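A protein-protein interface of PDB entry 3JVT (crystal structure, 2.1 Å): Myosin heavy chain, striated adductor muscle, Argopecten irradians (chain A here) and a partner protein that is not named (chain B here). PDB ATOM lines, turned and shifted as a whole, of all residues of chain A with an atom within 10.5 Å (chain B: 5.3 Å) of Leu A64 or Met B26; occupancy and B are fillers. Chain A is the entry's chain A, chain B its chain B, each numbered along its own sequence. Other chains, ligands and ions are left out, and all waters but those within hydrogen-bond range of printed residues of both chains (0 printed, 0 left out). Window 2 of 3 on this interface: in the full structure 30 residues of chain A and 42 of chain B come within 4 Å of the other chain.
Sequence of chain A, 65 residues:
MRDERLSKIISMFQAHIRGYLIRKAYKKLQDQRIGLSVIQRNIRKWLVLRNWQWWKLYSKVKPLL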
ATOM      1  N   TRP A  54       2.143 -13.758  24.294  1.00  0.00           N
ATOM      2  CA  TRP A  54       0.697 -13.734  24.355  1.00  0.00           C
ATOM      3  C   TRP A  54       0.212 -13.672  25.811  1.00  0.00           C
ATOM      4  O   TRP A  54      -0.787 -13.005  26.102  1.00  0.00           O
ATOM      5  CB  TRP A  54       0.090 -14.932  23.604  1.00  0.00           C
ATOM      6  CG  TRP A  54       0.038 -14.747  22.085  1.00  0.00           C
ATOM      7  CD1 TRP A  54       0.747 -15.441  21.148  1.00  0.00           C
ATOM      8  CD2 TRP A  54      -0.767 -13.814  21.359  1.00  0.00           C
ATOM      9  NE1 TRP A  54       0.428 -15.003  19.882  1.00  0.00           N
ATOM     10  CE2 TRP A  54      -0.501 -14.005  19.984  1.00  0.00           C
ATOM     11  CE3 TRP A  54      -1.696 -12.836  21.735  1.00  0.00           C
ATOM     12  CZ2 TRP A  54      -1.123 -13.254  18.986  1.00  0.00           C
ATOM     13  CZ3 TRP A  54      -2.315 -12.088  20.742  1.00  0.00           C
ATOM     14  CH2 TRP A  54      -2.024 -12.304  19.384  1.00  0.00           C
ATOM     15  N   LEU A  57       0.786 -10.129  27.028  1.00  0.00           N
ATOM     16  CA  LEU A  57      -0.258  -9.255  26.507  1.00  0.00           C
ATOM     17  C   LEU A  57      -1.579  -9.478  27.236  1.00  0.00           C
ATOM     18  O   LEU A  57      -2.218  -8.531  27.700  1.00  0.00           O
ATOM     19  CB  LEU A  57      -0.442  -9.478  25.005  1.00  0.00           C
ATOM     20  CG  LEU A  57      -1.657  -8.803  24.363  1.00  0.00           C
ATOM     21  CD1 LEU A  57      -1.371  -7.336  24.083  1.00  0.00           C
ATOM     22  CD2 LEU A  57      -2.064  -9.527  23.089  1.00  0.00           C
ATOM     23  N   TYR A  58      -1.952 -10.736  27.396  1.00  0.00           N
ATOM     24  CA  TYR A  58      -3.191 -11.068  28.076  1.00  0.00           C
ATOM     25  C   TYR A  58      -3.195 -10.538  29.505  1.00  0.00           C
ATOM     26  O   TYR A  58      -4.178  -9.955  29.956  1.00  0.00           O
ATOM     27  CB  TYR A  58      -3.379 -12.584  28.094  1.00  0.00           C
ATOM     28  CG  TYR A  58      -4.638 -13.032  28.791  1.00  0.00           C
ATOM     29  CD1 TYR A  58      -5.886 -12.617  28.345  1.00  0.00           C
ATOM     30  CD2 TYR A  58      -4.582 -13.890  29.883  1.00  0.00           C
ATOM     31  CE1 TYR A  58      -7.053 -13.047  28.970  1.00  0.00           C
ATOM     32  CE2 TYR A  58      -5.740 -14.328  30.510  1.00  0.00           C
ATOM     33  CZ  TYR A  58      -6.971 -13.901  30.050  1.00  0.00           C
ATOM     34  OH  TYR A  58      -8.119 -14.329  30.675  1.00  0.00           O
ATOM     35  N   SER A  59      -2.084 -10.732  30.207  1.00  0.00           N
ATOM     36  CA  SER A  59      -1.955 -10.297  31.585  1.00  0.00           C
ATOM     37  C   SER A  59      -2.061  -8.792  31.790  1.00  0.00           C
ATOM     38  O   SER A  59      -2.712  -8.340  32.732  1.00  0.00           O
ATOM     39  CB  SER A  59      -0.632 -10.794  32.178  1.00  0.00           C
ATOM     40  OG  SER A  59      -0.599 -12.210  32.237  1.00  0.00           O
ATOM     41  N   LYS A  60      -1.433  -8.020  30.905  1.00  0.00           N
ATOM     42  CA  LYS A  60      -1.470  -6.560  30.962  1.00  0.00           C
ATOM     43  C   LYS A  60      -2.851  -6.020  30.629  1.00  0.00           C
ATOM     44  O   LYS A  60      -3.226  -4.932  31.047  1.00  0.00           O
ATOM     45  CB  LYS A  60      -0.451  -5.954  29.996  1.00  0.00           C
ATOM     46  CG  LYS A  60       0.961  -5.901  30.533  1.00  0.00           C
ATOM     47  CD  LYS A  60       1.948  -5.405  29.493  1.00  0.00           C
ATOM     48  CE  LYS A  60       1.479  -5.719  28.086  1.00  0.00           C
ATOM     49  NZ  LYS A  60       2.613  -6.081  27.199  1.00  0.00           N
ATOM     50  N   VAL A  61      -3.603  -6.791  29.859  1.00  0.00           N
ATOM     51  CA  VAL A  61      -4.916  -6.356  29.387  1.00  0.00           C
ATOM     52  C   VAL A  61      -6.025  -6.623  30.411  1.00  0.00           C
ATOM     53  O   VAL A  61      -7.001  -5.876  30.494  1.00  0.00           O
ATOM     54  CB  VAL A  61      -5.298  -7.067  28.062  1.00  0.00           C
ATOM     55  CG1 VAL A  61      -6.815  -7.060  27.878  1.00  0.00           C
ATOM     56  CG2 VAL A  61      -4.626  -6.360  26.872  1.00  0.00           C
ATOM     57  N   LYS A  62      -5.869  -7.690  31.187  1.00  0.00           N
ATOM     58  CA  LYS A  62      -6.868  -8.077  32.180  1.00  0.00           C
ATOM     59  C   LYS A  62      -7.477  -6.972  33.044  1.00  0.00           C
ATOM     60  O   LYS A  62      -8.701  -6.847  33.126  1.00  0.00           O
ATOM     61  CB  LYS A  62      -6.303  -9.164  33.090  1.00  0.00           C
ATOM     62  CG  LYS A  62      -6.537 -10.565  32.576  1.00  0.00           C
ATOM     63  CD  LYS A  62      -6.043 -11.607  33.566  1.00  0.00           C
ATOM     64  CE  LYS A  62      -6.548 -12.988  33.186  1.00  0.00           C
ATOM     65  NZ  LYS A  62      -5.850 -14.090  33.912  1.00  0.00           N
ATOM     66  N   PRO A  63      -6.638  -6.154  33.699  1.00  0.00           N
ATOM     67  CA  PRO A  63      -7.108  -5.068  34.562  1.00  0.00           C
ATOM     68  C   PRO A  63      -8.169  -4.163  33.939  1.00  0.00           C
ATOM     69  O   PRO A  63      -8.898  -3.472  34.649  1.00  0.00           O
ATOM     70  CB  PRO A  63      -5.830  -4.297  34.873  1.00  0.00           C
ATOM     71  CG  PRO A  63      -4.795  -5.381  34.880  1.00  0.00           C
ATOM     72  CD  PRO A  63      -5.163  -6.180  33.661  1.00  0.00           C
ATOM     73  N   LEU A  64      -8.247  -4.166  32.616  1.00  0.00           N
ATOM     74  CA  LEU A  64      -9.202  -3.326  31.915  1.00  0.00           C
ATOM     75  C   LEU A  64     -10.524  -4.040  31.625  1.00  0.00           C
ATOM     76  O   LEU A  64     -11.413  -3.462  30.997  1.00  0.00           O
ATOM     77  CB  LEU A  64      -8.590  -2.836  30.594  1.00  0.00           C
ATOM     78  CG  LEU A  64      -7.150  -2.300  30.622  1.00  0.00           C
ATOM     79  CD1 LEU A  64      -6.766  -1.793  29.235  1.00  0.00           C
ATOM     80  CD2 LEU A  64      -7.023  -1.186  31.660  1.00  0.00           C
ATOM     81  N   LEU A  65     -10.658  -5.286  32.080  1.00  0.00           N
ATOM     82  CA  LEU A  65     -11.872  -6.064  31.827  1.00  0.00           C
ATOM     83  C   LEU A  65     -12.999  -5.903  32.853  1.00  0.00           C
ATOM     84  O   LEU A  65     -12.786  -5.210  33.870  1.00  0.00           O
ATOM     85  CB  LEU A  65     -11.522  -7.549  31.696  1.00  0.00           C
ATOM     86  CG  LEU A  65     -10.505  -7.956  30.623  1.00  0.00           C
ATOM     87  CD1 LEU A  65     -10.484  -9.469  30.533  1.00  0.00           C
ATOM     88  CD2 LEU A  65     -10.872  -7.357  29.272  1.00  0.00           C
ATOM     89  OXT LEU A  65     -14.081  -6.486  32.623  1.00  0.00           O
ATOM     90  N   GLU B  22     -13.185 -11.254  26.548  1.00  0.00           N
ATOM     91  CA  GLU B  22     -13.189  -9.819  26.805  1.00  0.00           C
ATOM     92  C   GLU B  22     -11.819  -9.199  26.570  1.00  0.00           C
ATOM     93  O   GLU B  22     -11.708  -8.021  26.241  1.00  0.00           O
ATOM     94  CB  GLU B  22     -13.658  -9.544  28.236  1.00  0.00           C
ATOM     95  CG  GLU B  22     -15.159  -9.687  28.436  1.00  0.00           C
ATOM     96  CD  GLU B  22     -15.544  -9.772  29.899  1.00  0.00           C
ATOM     97  OE1 GLU B  22     -15.233  -8.826  30.656  1.00  0.00           O
ATOM     98  OE2 GLU B  22     -16.160 -10.788  30.293  1.00  0.00           O
ATOM     99  N   ALA B  23     -10.778  -9.999  26.754  1.00  0.00           N
ATOM    100  CA  ALA B  23      -9.424  -9.537  26.539  1.00  0.00           C
ATOM    101  C   ALA B  23      -9.333  -9.429  25.034  1.00  0.00           C
ATOM    102  O   ALA B  23      -8.833  -8.444  24.496  1.00  0.00           O
ATOM    103  CB  ALA B  23      -8.427 -10.561  27.051  1.00  0.00           C
ATOM    104  N   PHE B  24      -9.835 -10.459  24.363  1.00  0.00           N
ATOM    105  CA  PHE B  24      -9.818 -10.508  22.918  1.00  0.00           C
ATOM    106  C   PHE B  24     -10.443  -9.260  22.341  1.00  0.00           C
ATOM    107  O   PHE B  24      -9.906  -8.663  21.406  1.00  0.00           O
ATOM    108  CB  PHE B  24     -10.590 -11.714  22.385  1.00  0.00           C
ATOM    109  CG  PHE B  24     -10.596 -11.794  20.885  1.00  0.00           C
ATOM    110  CD1 PHE B  24      -9.615 -12.522  20.211  1.00  0.00           C
ATOM    111  CD2 PHE B  24     -11.525 -11.066  20.143  1.00  0.00           C
ATOM    112  CE1 PHE B  24      -9.557 -12.518  18.822  1.00  0.00           C
ATOM    113  CE2 PHE B  24     -11.477 -11.052  18.758  1.00  0.00           C
ATOM    114  CZ  PHE B  24     -10.488 -11.779  18.091  1.00  0.00           C
ATOM    115  N   SER B  25     -11.585  -8.869  22.896  1.00  0.00           N
ATOM    116  CA  SER B  25     -12.282  -7.682  22.416  1.00  0.00           C
ATOM    117  C   SER B  25     -11.408  -6.440  22.547  1.00  0.00           C
ATOM    118  O   SER B  25     -11.344  -5.638  21.620  1.00  0.00           O
ATOM    119  CB  SER B  25     -13.616  -7.491  23.160  1.00  0.00           C
ATOM    120  OG  SER B  25     -14.598  -8.410  22.691  1.00  0.00           O
ATOM    121  N   MET B  26     -10.735  -6.271  23.684  1.00  0.00           N
ATOM    122  CA  MET B  26      -9.863  -5.106  23.859  1.00  0.00           C
ATOM    123  C   MET B  26      -8.633  -5.160  22.955  1.00  0.00           C
ATOM    124  O   MET B  26      -8.239  -4.153  22.369  1.00  0.00           O
ATOM    125  CB  MET B  26      -9.417  -4.979  25.305  1.00  0.00           C
ATOM    126  CG  MET B  26     -10.505  -4.566  26.240  1.00  0.00           C
ATOM    127  SD  MET B  26      -9.780  -3.594  27.549  1.00  0.00           S
ATOM    128  CE  MET B  26     -10.480  -2.024  27.158  1.00  0.00           C
ATOM    129  N   ILE B  27      -8.021  -6.339  22.862  1.00  0.00           N
ATOM    130  CA  ILE B  27      -6.868  -6.589  21.997  1.00  0.00           C
ATOM    131  C   ILE B  27      -7.168  -6.257  20.527  1.00  0.00           C
ATOM    132  O   ILE B  27      -6.318  -5.726  19.807  1.00  0.00           O
ATOM    133  CB  ILE B  27      -6.402  -8.062  22.112  1.00  0.00           C
ATOM    134  CG1 ILE B  27      -5.822  -8.309  23.510  1.00  0.00           C
ATOM    135  CG2 ILE B  27      -5.369  -8.378  21.041  1.00  0.00           C
ATOM    136  CD1 ILE B  27      -5.422  -9.766  23.768  1.00  0.00           C
ATOM    137  N   ASP B  28      -8.391  -6.569  20.094  1.00  0.00           N
ATOM    138  CA  ASP B  28      -8.825  -6.305  18.728  1.00  0.00           C
ATOM    139  C   ASP B  28      -9.269  -4.843  18.637  1.00  0.00           C
ATOM    140  O   ASP B  28     -10.459  -4.528  18.560  1.00  0.00           O
ATOM    141  CB  ASP B  28      -9.971  -7.275  18.359  1.00  0.00           C
ATOM    142  CG  ASP B  28     -10.697  -6.891  17.089  1.00  0.00           C
ATOM    143  OD1 ASP B  28     -10.116  -6.212  16.227  1.00  0.00           O
ATOM    144  OD2 ASP B  28     -11.864  -7.294  16.945  1.00  0.00           O
ATOM    145  N   VAL B  29      -8.263  -3.961  18.660  1.00  0.00           N
ATOM    146  CA  VAL B  29      -8.430  -2.508  18.577  1.00  0.00           C
ATOM    147  C   VAL B  29      -9.461  -1.990  17.588  1.00  0.00           C
ATOM    148  O   VAL B  29     -10.414  -1.314  17.979  1.00  0.00           O
ATOM    149  CB  VAL B  29      -7.050  -1.801  18.286  1.00  0.00           C
ATOM    150  CG1 VAL B  29      -7.278  -0.326  17.986  1.00  0.00           C
ATOM    151  CG2 VAL B  29      -6.126  -1.967  19.482  1.00  0.00           C
ATOM    152  N   ILE B  43      -2.654  -1.778  21.104  1.00  0.00           N
ATOM    153  CA  ILE B  43      -3.018  -2.032  22.488  1.00  0.00           C
ATOM    154  C   ILE B  43      -1.766  -2.103  23.364  1.00  0.00           C
ATOM    155  O   ILE B  43      -1.778  -1.652  24.505  1.00  0.00           O
ATOM    156  CB  ILE B  43      -3.845  -3.330  22.640  1.00  0.00           C
ATOM    157  CG1 ILE B  43      -4.417  -3.397  24.060  1.00  0.00           C
ATOM    158  CG2 ILE B  43      -2.980  -4.541  22.300  1.00  0.00           C
ATOM    159  CD1 ILE B  43      -5.206  -2.164  24.454  1.00  0.00           C
ATOM    160  N   GLN B  46      -0.399   1.256  24.062  1.00  0.00           N
ATOM    161  CA  GLN B  46      -1.338   1.852  24.991  1.00  0.00           C
ATOM    162  C   GLN B  46      -0.970   1.442  26.420  1.00  0.00           C
ATOM    163  O   GLN B  46      -0.989   2.260  27.342  1.00  0.00           O
ATOM    164  CB  GLN B  46      -2.749   1.364  24.647  1.00  0.00           C
ATOM    165  CG  GLN B  46      -3.838   2.063  25.413  1.00  0.00           C
ATOM    166  CD  GLN B  46      -5.209   1.466  25.172  1.00  0.00           C
ATOM    167  OE1 GLN B  46      -5.612   1.221  24.026  1.00  0.00           O
ATOM    168  NE2 GLN B  46      -5.945   1.238  26.256  1.00  0.00           N
ATOM    169  N   LEU B  47      -0.628   0.176  26.586  1.00  0.00           N
ATOM    170  CA  LEU B  47      -0.323  -0.353  27.903  1.00  0.00           C
ATOM    171  C   LEU B  47       1.114  -0.324  28.364  1.00  0.00           C
ATOM    172  O   LEU B  47       1.405  -0.751  29.478  1.00  0.00           O
ATOM    173  CB  LEU B  47      -0.853  -1.776  27.997  1.00  0.00           C
ATOM    174  CG  LEU B  47      -2.347  -1.929  27.699  1.00  0.00           C
ATOM    175  CD1 LEU B  47      -2.687  -3.375  27.869  1.00  0.00           C
ATOM    176  CD2 LEU B  47      -3.206  -1.074  28.624  1.00  0.00           C
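Of the 11 printed residues of chain B, 6 touch a printed residue of chain A. Hydrophobic or aromatic side chains of chain A that line the printed part of chain B: Leu A57, Tyr A58, Val A61, Leu A64 and Leu A65. Among the printed residues, 10 pairs touch across the chains. Among the printed residues, no Asp or Glu carboxylate lies within 4 Å of a Lys or Arg side-chain nitrogen of the other chain.
Printed residues of chain B within 4 Å of Tyr A58: Ala B23 (3.4 Å). Ser A59 touches none of the printed residues of chain B. Of the printed residues of chain B, Lys A60 touches Leu B47 (3.6 Å). Printed residues of chain B within 4 Å of Val A61: Ala B23 (3.8 Å) and Leu B47 (3.7 Å). Of the printed residues of chain B, Leu A64 touches Met B26 (3.4 Å) and Leu B47 (3.7 Å). No residue of chain A comes within 4 Å of Ser B25. Met B26 touches just one residue of chain A: Leu A64 (3.4 Å). Asp B28 touches none of the printed residues of chain A. Of the printed residues of chain A, Ile B43 touches Leu A57 (3.7 Å). The nearest residue of chain B that does not touch Leu A64 is Gln B46 (4.3 Å). The nearest printed residue of chain B that does not touch Val A61 is Ile B27 (4.1 Å).
The chain-end carboxylate of Leu A65 sits close to the side-chain carboxylate of Glu B22 (3.3 Å).
Ile B27 touches Leu A57. Leu A57 touches Ile B43 (CD1 to CG2, 3.7 Å). Ala B23 touches Tyr A58. Lys A60 touches Leu B47 (O to CD1, 3.6 Å). CA of Ala B23 touches CG1 of Val A61 (3.8 Å). CG2 of Val A61 touches CD1 of Leu B47 (3.7 Å). Met B26 touches Leu A64 (SD to CB, 3.4 Å). Leu B47 touches Leu A64 (CD2 to CD1, 3.7 Å). Ala B23 touches Leu A65 (N to CD2, 3.7 Å).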
